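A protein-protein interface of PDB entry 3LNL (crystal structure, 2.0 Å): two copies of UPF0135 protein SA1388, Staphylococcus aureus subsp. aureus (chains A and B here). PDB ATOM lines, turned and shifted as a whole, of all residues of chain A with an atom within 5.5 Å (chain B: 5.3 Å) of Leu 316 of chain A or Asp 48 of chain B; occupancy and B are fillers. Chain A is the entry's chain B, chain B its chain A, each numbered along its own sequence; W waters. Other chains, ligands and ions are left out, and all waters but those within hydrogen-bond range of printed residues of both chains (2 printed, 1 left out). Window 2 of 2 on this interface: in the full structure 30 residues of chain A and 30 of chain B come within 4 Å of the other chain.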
ATOM      1  N   LYS A 311      36.184   4.985   6.426  1.00  0.00           N
ATOM      2  CA  LYS A 311      34.744   5.116   6.263  1.00  0.00           C
ATOM      3  C   LYS A 311      34.053   5.764   7.471  1.00  0.00           C
ATOM      4  O   LYS A 311      34.579   5.775   8.593  1.00  0.00           O
ATOM      5  CB  LYS A 311      34.128   3.758   5.992  1.00  0.00           C
ATOM      6  CG  LYS A 311      34.653   3.209   4.638  1.00  0.00           C
ATOM      7  CD  LYS A 311      34.019   1.929   4.205  1.00  0.00           C
ATOM      8  CE  LYS A 311      33.943   0.944   5.348  1.00  0.00           C
ATOM      9  NZ  LYS A 311      33.310  -0.344   4.869  1.00  0.00           N
ATOM     10  N   HIS A 312      32.885   6.343   7.192  1.00  0.00           N
ATOM     11  CA  HIS A 312      32.097   7.097   8.182  1.00  0.00           C
ATOM     12  C   HIS A 312      31.989   6.463   9.544  1.00  0.00           C
ATOM     13  O   HIS A 312      32.348   7.078  10.536  1.00  0.00           O
ATOM     14  CB  HIS A 312      30.684   7.321   7.623  1.00  0.00           C
ATOM     15  CG  HIS A 312      29.778   8.030   8.558  1.00  0.00           C
ATOM     16  ND1 HIS A 312      29.894   9.372   8.827  1.00  0.00           N
ATOM     17  CD2 HIS A 312      28.766   7.563   9.347  1.00  0.00           C
ATOM     18  CE1 HIS A 312      28.963   9.718   9.710  1.00  0.00           C
ATOM     19  NE2 HIS A 312      28.271   8.636  10.052  1.00  0.00           N
ATOM     20  N   HIS A 313      31.438   5.245   9.610  1.00  0.00           N
ATOM     21  CA  HIS A 313      31.140   4.652  10.898  1.00  0.00           C
ATOM     22  C   HIS A 313      32.416   4.346  11.672  1.00  0.00           C
ATOM     23  O   HIS A 313      32.428   4.443  12.896  1.00  0.00           O
ATOM     24  CB  HIS A 313      30.247   3.413  10.773  1.00  0.00           C
ATOM     25  CG  HIS A 313      28.815   3.758  10.530  1.00  0.00           C
ATOM     26  ND1 HIS A 313      28.010   4.302  11.507  1.00  0.00           N
ATOM     27  CD2 HIS A 313      28.067   3.700   9.401  1.00  0.00           C
ATOM     28  CE1 HIS A 313      26.816   4.547  10.988  1.00  0.00           C
ATOM     29  NE2 HIS A 313      26.820   4.168   9.718  1.00  0.00           N
ATOM     30  N   ASP A 314      33.495   3.990  10.978  1.00  0.00           N
ATOM     31  CA  ASP A 314      34.752   3.789  11.693  1.00  0.00           C
ATOM     32  C   ASP A 314      35.364   5.093  12.226  1.00  0.00           C
ATOM     33  O   ASP A 314      35.939   5.101  13.327  1.00  0.00           O
ATOM     34  CB  ASP A 314      35.770   3.044  10.837  1.00  0.00           C
ATOM     35  CG  ASP A 314      35.300   1.620  10.522  1.00  0.00           C
ATOM     36  OD1 ASP A 314      34.766   0.899  11.413  1.00  0.00           O
ATOM     37  OD2 ASP A 314      35.451   1.295   9.361  1.00  0.00           O
ATOM     38  N   ALA A 315      35.238   6.158  11.445  1.00  0.00           N
ATOM     39  CA  ALA A 315      35.641   7.490  11.883  1.00  0.00           C
ATOM     40  C   ALA A 315      34.783   7.947  13.078  1.00  0.00           C
ATOM     41  O   ALA A 315      35.298   8.552  14.024  1.00  0.00           O
ATOM     42  CB  ALA A 315      35.524   8.503  10.739  1.00  0.00           C
ATOM     43  N   LEU A 316      33.466   7.744  12.981  1.00  0.00           N
ATOM     44  CA  LEU A 316      32.552   8.057  14.097  1.00  0.00           C
ATOM     45  C   LEU A 316      32.963   7.355  15.410  1.00  0.00           C
ATOM     46  O   LEU A 316      33.036   7.962  16.456  1.00  0.00           O
ATOM     47  CB  LEU A 316      31.107   7.680  13.736  1.00  0.00           C
ATOM     48  CG  LEU A 316      30.018   8.353  14.591  1.00  0.00           C
ATOM     49  CD1 LEU A 316      30.019   9.861  14.293  1.00  0.00           C
ATOM     50  CD2 LEU A 316      28.637   7.731  14.316  1.00  0.00           C
ATOM     51  N   ASP A 317      33.185   6.046  15.330  1.00  0.00           N
ATOM     52  CA  ASP A 317      33.673   5.255  16.458  1.00  0.00           C
ATOM     53  C   ASP A 317      34.983   5.830  17.023  1.00  0.00           C
ATOM     54  O   ASP A 317      35.102   6.059  18.260  1.00  0.00           O
ATOM     55  CB  ASP A 317      33.898   3.790  16.042  1.00  0.00           C
ATOM     56  CG  ASP A 317      32.597   3.090  15.735  1.00  0.00           C
ATOM     57  OD1 ASP A 317      31.542   3.687  15.975  1.00  0.00           O
ATOM     58  OD2 ASP A 317      32.616   1.970  15.220  1.00  0.00           O
ATOM     59  N   ALA A 318      35.948   6.058  16.138  1.00  0.00           N
ATOM     60  CA  ALA A 318      37.241   6.635  16.544  1.00  0.00           C
ATOM     61  C   ALA A 318      37.065   7.976  17.288  1.00  0.00           C
ATOM     62  O   ALA A 318      37.615   8.160  18.379  1.00  0.00           O
ATOM     63  CB  ALA A 318      38.172   6.803  15.325  1.00  0.00           C
ATOM     64  N   LYS A 319      36.227   8.856  16.733  1.00  0.00           N
ATOM     65  CA  LYS A 319      35.971  10.159  17.344  1.00  0.00           C
ATOM     66  C   LYS A 319      35.437  10.000  18.780  1.00  0.00           C
ATOM     67  O   LYS A 319      35.977  10.610  19.745  1.00  0.00           O
ATOM     68  CB  LYS A 319      34.989  10.992  16.513  1.00  0.00           C
ATOM     69  CG  LYS A 319      34.852  12.456  17.045  1.00  0.00           C
ATOM     70  CD  LYS A 319      34.380  13.441  15.966  1.00  0.00           C
ATOM     71  CE  LYS A 319      34.216  14.876  16.530  1.00  0.00           C
ATOM     72  NZ  LYS A 319      35.564  15.578  16.557  1.00  0.00           N
ATOM     73  N   ILE A 320      34.406   9.187  18.938  1.00  0.00           N
ATOM     74  CA  ILE A 320      33.800   9.053  20.253  1.00  0.00           C
ATOM     75  C   ILE A 320      34.768   8.429  21.265  1.00  0.00           C
ATOM     76  O   ILE A 320      34.743   8.747  22.441  1.00  0.00           O
ATOM     77  CB  ILE A 320      32.447   8.303  20.190  1.00  0.00           C
ATOM     78  CG1 ILE A 320      31.575   8.749  21.406  1.00  0.00           C
ATOM     79  CG2 ILE A 320      32.640   6.809  20.243  1.00  0.00           C
ATOM     80  CD1 ILE A 320      30.113   8.302  21.371  1.00  0.00           C
ATOM     81  N   HIS A 321      35.666   7.563  20.803  1.00  0.00           N
ATOM     82  CA  HIS A 321      36.638   6.970  21.697  1.00  0.00           C
ATOM     83  C   HIS A 321      37.932   7.784  21.832  1.00  0.00           C
ATOM     84  O   HIS A 321      38.828   7.382  22.522  1.00  0.00           O
ATOM     85  CB  HIS A 321      36.973   5.558  21.234  1.00  0.00           C
ATOM     86  CG  HIS A 321      35.821   4.606  21.315  1.00  0.00           C
ATOM     87  ND1 HIS A 321      35.184   4.301  22.503  1.00  0.00           N
ATOM     88  CD2 HIS A 321      35.189   3.904  20.351  1.00  0.00           C
ATOM     89  CE1 HIS A 321      34.190   3.468  22.252  1.00  0.00           C
ATOM     90  NE2 HIS A 321      34.173   3.215  20.951  1.00  0.00           N
ATOM     91  N   ALA B  46      17.830  13.757  13.332  1.00  0.00           N
ATOM     92  CA  ALA B  46      19.287  13.586  13.408  1.00  0.00           C
ATOM     93  C   ALA B  46      19.757  12.524  12.446  1.00  0.00           C
ATOM     94  O   ALA B  46      18.976  11.654  12.068  1.00  0.00           O
ATOM     95  CB  ALA B  46      19.761  13.236  14.864  1.00  0.00           C
ATOM     96  N   LEU B  47      21.009  12.650  11.969  1.00  0.00           N
ATOM     97  CA  LEU B  47      21.616  11.588  11.208  1.00  0.00           C
ATOM     98  C   LEU B  47      22.174  10.567  12.211  1.00  0.00           C
ATOM     99  O   LEU B  47      21.705   9.412  12.265  1.00  0.00           O
ATOM    100  CB  LEU B  47      22.731  12.105  10.274  1.00  0.00           C
ATOM    101  CG  LEU B  47      23.594  11.082   9.517  1.00  0.00           C
ATOM    102  CD1 LEU B  47      22.683  10.213   8.570  1.00  0.00           C
ATOM    103  CD2 LEU B  47      24.705  11.801   8.723  1.00  0.00           C
ATOM    104  N   ASP B  48      23.196  11.004  12.956  1.00  0.00           N
ATOM    105  CA  ASP B  48      23.749  10.308  14.070  1.00  0.00           C
ATOM    106  C   ASP B  48      23.357  11.010  15.377  1.00  0.00           C
ATOM    107  O   ASP B  48      23.468  12.242  15.517  1.00  0.00           O
ATOM    108  CB  ASP B  48      25.270  10.231  13.942  1.00  0.00           C
ATOM    109  CG  ASP B  48      25.713   9.269  12.852  1.00  0.00           C
ATOM    110  OD1 ASP B  48      25.363   8.069  12.948  1.00  0.00           O
ATOM    111  OD2 ASP B  48      26.420   9.706  11.903  1.00  0.00           O
ATOM    112  N   CYS B  49      22.902  10.203  16.325  1.00  0.00           N
ATOM    113  CA  CYS B  49      22.595  10.689  17.647  1.00  0.00           C
ATOM    114  C   CYS B  49      23.853  10.758  18.495  1.00  0.00           C
ATOM    115  O   CYS B  49      24.162   9.837  19.182  1.00  0.00           O
ATOM    116  CB  CYS B  49      21.525   9.813  18.294  1.00  0.00           C
ATOM    117  SG  CYS B  49      20.984  10.518  19.896  1.00  0.00           S
ATOM    118  N   THR B  50      24.592  11.862  18.386  1.00  0.00           N
ATOM    119  CA  THR B  50      25.791  12.097  19.163  1.00  0.00           C
ATOM    120  C   THR B  50      25.442  12.686  20.540  1.00  0.00           C
ATOM    121  O   THR B  50      24.302  13.144  20.792  1.00  0.00           O
ATOM    122  CB  THR B  50      26.715  13.117  18.449  1.00  0.00           C
ATOM    123  OG1 THR B  50      26.089  14.408  18.418  1.00  0.00           O
ATOM    124  CG2 THR B  50      27.095  12.607  17.013  1.00  0.00           C
ATOM    125  N   VAL B  53      23.952  16.053  20.088  1.00  0.00           N
ATOM    126  CA  VAL B  53      22.535  16.031  19.660  1.00  0.00           C
ATOM    127  C   VAL B  53      21.625  15.810  20.876  1.00  0.00           C
ATOM    128  O   VAL B  53      20.574  16.439  20.983  1.00  0.00           O
ATOM    129  CB  VAL B  53      22.270  14.956  18.589  1.00  0.00           C
ATOM    130  CG1 VAL B  53      20.771  14.783  18.328  1.00  0.00           C
ATOM    131  CG2 VAL B  53      23.026  15.287  17.268  1.00  0.00           C
ATOM    132  N   SER B  67      16.643   9.492  14.687  1.00  0.00           N
ATOM    133  CA  SER B  67      17.881   9.451  13.917  1.00  0.00           C
ATOM    134  C   SER B  67      17.694   8.475  12.752  1.00  0.00           C
ATOM    135  O   SER B  67      16.790   7.613  12.743  1.00  0.00           O
ATOM    136  CB  SER B  67      19.065   9.007  14.807  1.00  0.00           C
ATOM    137  OG  SER B  67      18.957   7.610  15.171  1.00  0.00           O
ATOM    138  N   HIS B  69      20.659   6.783  11.584  1.00  0.00           N
ATOM    139  CA  HIS B  69      21.568   5.699  12.020  1.00  0.00           C
ATOM    140  C   HIS B  69      21.211   5.200  13.416  1.00  0.00           C
ATOM    141  O   HIS B  69      20.958   6.016  14.299  1.00  0.00           O
ATOM    142  CB  HIS B  69      23.005   6.137  12.027  1.00  0.00           C
ATOM    143  CG  HIS B  69      23.565   6.397  10.665  1.00  0.00           C
ATOM    144  ND1 HIS B  69      24.602   7.278  10.452  1.00  0.00           N
ATOM    145  CD2 HIS B  69      23.264   5.864   9.452  1.00  0.00           C
ATOM    146  CE1 HIS B  69      24.897   7.297   9.162  1.00  0.00           C
ATOM    147  NE2 HIS B  69      24.158   6.391   8.542  1.00  0.00           N
ATOM    148  N   TYR B  84      29.957   5.378  23.514  1.00  0.00           N
ATOM    149  CA  TYR B  84      28.537   5.324  23.208  1.00  0.00           C
ATOM    150  C   TYR B  84      27.668   5.136  24.476  1.00  0.00           C
ATOM    151  O   TYR B  84      26.530   5.557  24.490  1.00  0.00           O
ATOM    152  CB  TYR B  84      28.205   4.230  22.172  1.00  0.00           C
ATOM    153  CG  TYR B  84      28.699   4.542  20.796  1.00  0.00           C
ATOM    154  CD1 TYR B  84      29.784   3.846  20.241  1.00  0.00           C
ATOM    155  CD2 TYR B  84      28.101   5.531  20.039  1.00  0.00           C
ATOM    156  CE1 TYR B  84      30.252   4.146  18.972  1.00  0.00           C
ATOM    157  CE2 TYR B  84      28.551   5.856  18.777  1.00  0.00           C
ATOM    158  CZ  TYR B  84      29.632   5.154  18.242  1.00  0.00           C
ATOM    159  OH  TYR B  84      30.059   5.498  17.001  1.00  0.00           O
ATOM    160  N   THR B 364      27.605  16.666  12.565  1.00  0.00           N
ATOM    161  CA  THR B 364      28.103  15.514  13.288  1.00  0.00           C
ATOM    162  C   THR B 364      29.128  14.699  12.474  1.00  0.00           C
ATOM    163  O   THR B 364      29.521  13.595  12.870  1.00  0.00           O
ATOM    164  CB  THR B 364      26.937  14.606  13.726  1.00  0.00           C
ATOM    165  OG1 THR B 364      26.183  14.228  12.564  1.00  0.00           O
ATOM    166  CG2 THR B 364      25.988  15.356  14.804  1.00  0.00           C
ATOM    167  N   PRO B 366      32.316  13.090  11.633  1.00  0.00           N
ATOM    168  CA  PRO B 366      33.600  12.903  12.361  1.00  0.00           C
ATOM    169  C   PRO B 366      34.832  13.453  11.600  1.00  0.00           C
ATOM    170  O   PRO B 366      35.858  13.694  12.182  1.00  0.00           O
ATOM    171  CB  PRO B 366      33.681  11.397  12.510  1.00  0.00           C
ATOM    172  CG  PRO B 366      32.863  10.858  11.339  1.00  0.00           C
ATOM    173  CD  PRO B 366      31.705  11.814  11.249  1.00  0.00           C
HETATM  174  O   HOH W   1      36.892  15.203  14.065  1.00  0.00           O
HETATM  175  O   HOH W   2      29.131   3.991  14.117  1.00  0.00           O
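The side-chain hydroxyl (OH) of Tyr 84 of chain B lies within hydrogen-bond range of the side-chain carboxylate (OD1) of Asp 317 of chain A (2.6 Å). OD2 of Asp 48 of chain B sits at hydrogen-bond distance from NE2 of His 312 of chain A, 2.8 Å away.
The side-chain hydroxyl (OG) of Ser 67 of chain B sits at hydrogen-bond distance from the backbone carbonyl oxygen (O) of His 69 of chain B, 2.7 Å away. A ring nitrogen (ND1) of His 69 of chain B is in hydrogen-bond range of the side-chain carboxylate (OD1) of Asp 48 of chain B, 2.7 Å away. O of Leu 47 of chain B is in hydrogen-bond range of N of His 69 of chain B.
Among the printed residues, merely in contact across the chains: His 312 of chain A with His 69 of chain B, His 312 of chain A with Pro 366 of chain B, His 313 of chain A with His 69 of chain B, Ala 315 of chain A with Pro 366 of chain B, Leu 316 of chain A with Asp 48 of chain B, Leu 316 of chain A with Tyr 84 of chain B, Leu 316 of chain A with Pro 366 of chain B, Lys 319 of chain A with Pro 366 of chain B and Ile 320 of chain A with Tyr 84 of chain B.
Of chain B, only Asp 48, Tyr 84 and Pro 366 come within 4 Å of Leu 316 of chain A. Of chain A, only His 312 and Leu 316 come within 4 Å of Asp 48 of chain B. Of the printed residues of chain A, His 69 of chain B touches His 312 (3.7 Å) and His 313 (3.6 Å). Of the printed residues of chain B, Asp 317 of chain A touches Tyr 84. Of the printed residues of chain A, Tyr 84 of chain B touches Leu 316 (3.7 Å), Asp 317 (2.6 Å) and Ile 320 (3.6 Å). Of the printed residues of chain B, His 313 of chain A touches His 69. The nearest residue of chain B that does not touch Leu 316 of chain A is Thr 364 of chain B (4.03 Å). The nearest residue of chain A that does not touch Asp 48 of chain B is His 313 of chain A (4.3 Å).
Printed residues of chain A that touch a printed residue of chain B: His 312, His 313, Ala 315, Leu 316, Asp 317, Lys 319 and Ile 320. Hydrophobic or aromatic side chains of chain A within 4 Å of the printed part of chain B: His 312, His 313, Ala 315, Leu 316 and Ile 320. Hydrophobic or aromatic side chains of chain B that line the printed part of chain A: His 69, Tyr 84 and Pro 366. Among the printed residues, 11 pairs touch across the chains. Among the printed residues, no Asp or Glu carboxylate lies within 4 Å of a Lys or Arg side-chain nitrogen of the other chain.
No position is printed for both chains. Of the 11 pairs that touch across the chains among the printed residues, none has its exchanged pair printed and touching as well.
Water W1 lies within hydrogen-bond range of O of Pro 366 of chain B and NZ of Lys 319 of chain A. Water W2 lies within hydrogen-bond range of a ring nitrogen (ND1) of His 313 of chain A (2.9 Å), the side-chain carboxylate of Asp 317 of chain A (3.1 Å) and the side-chain hydroxyl of Tyr 84 of chain B (3.4 Å).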
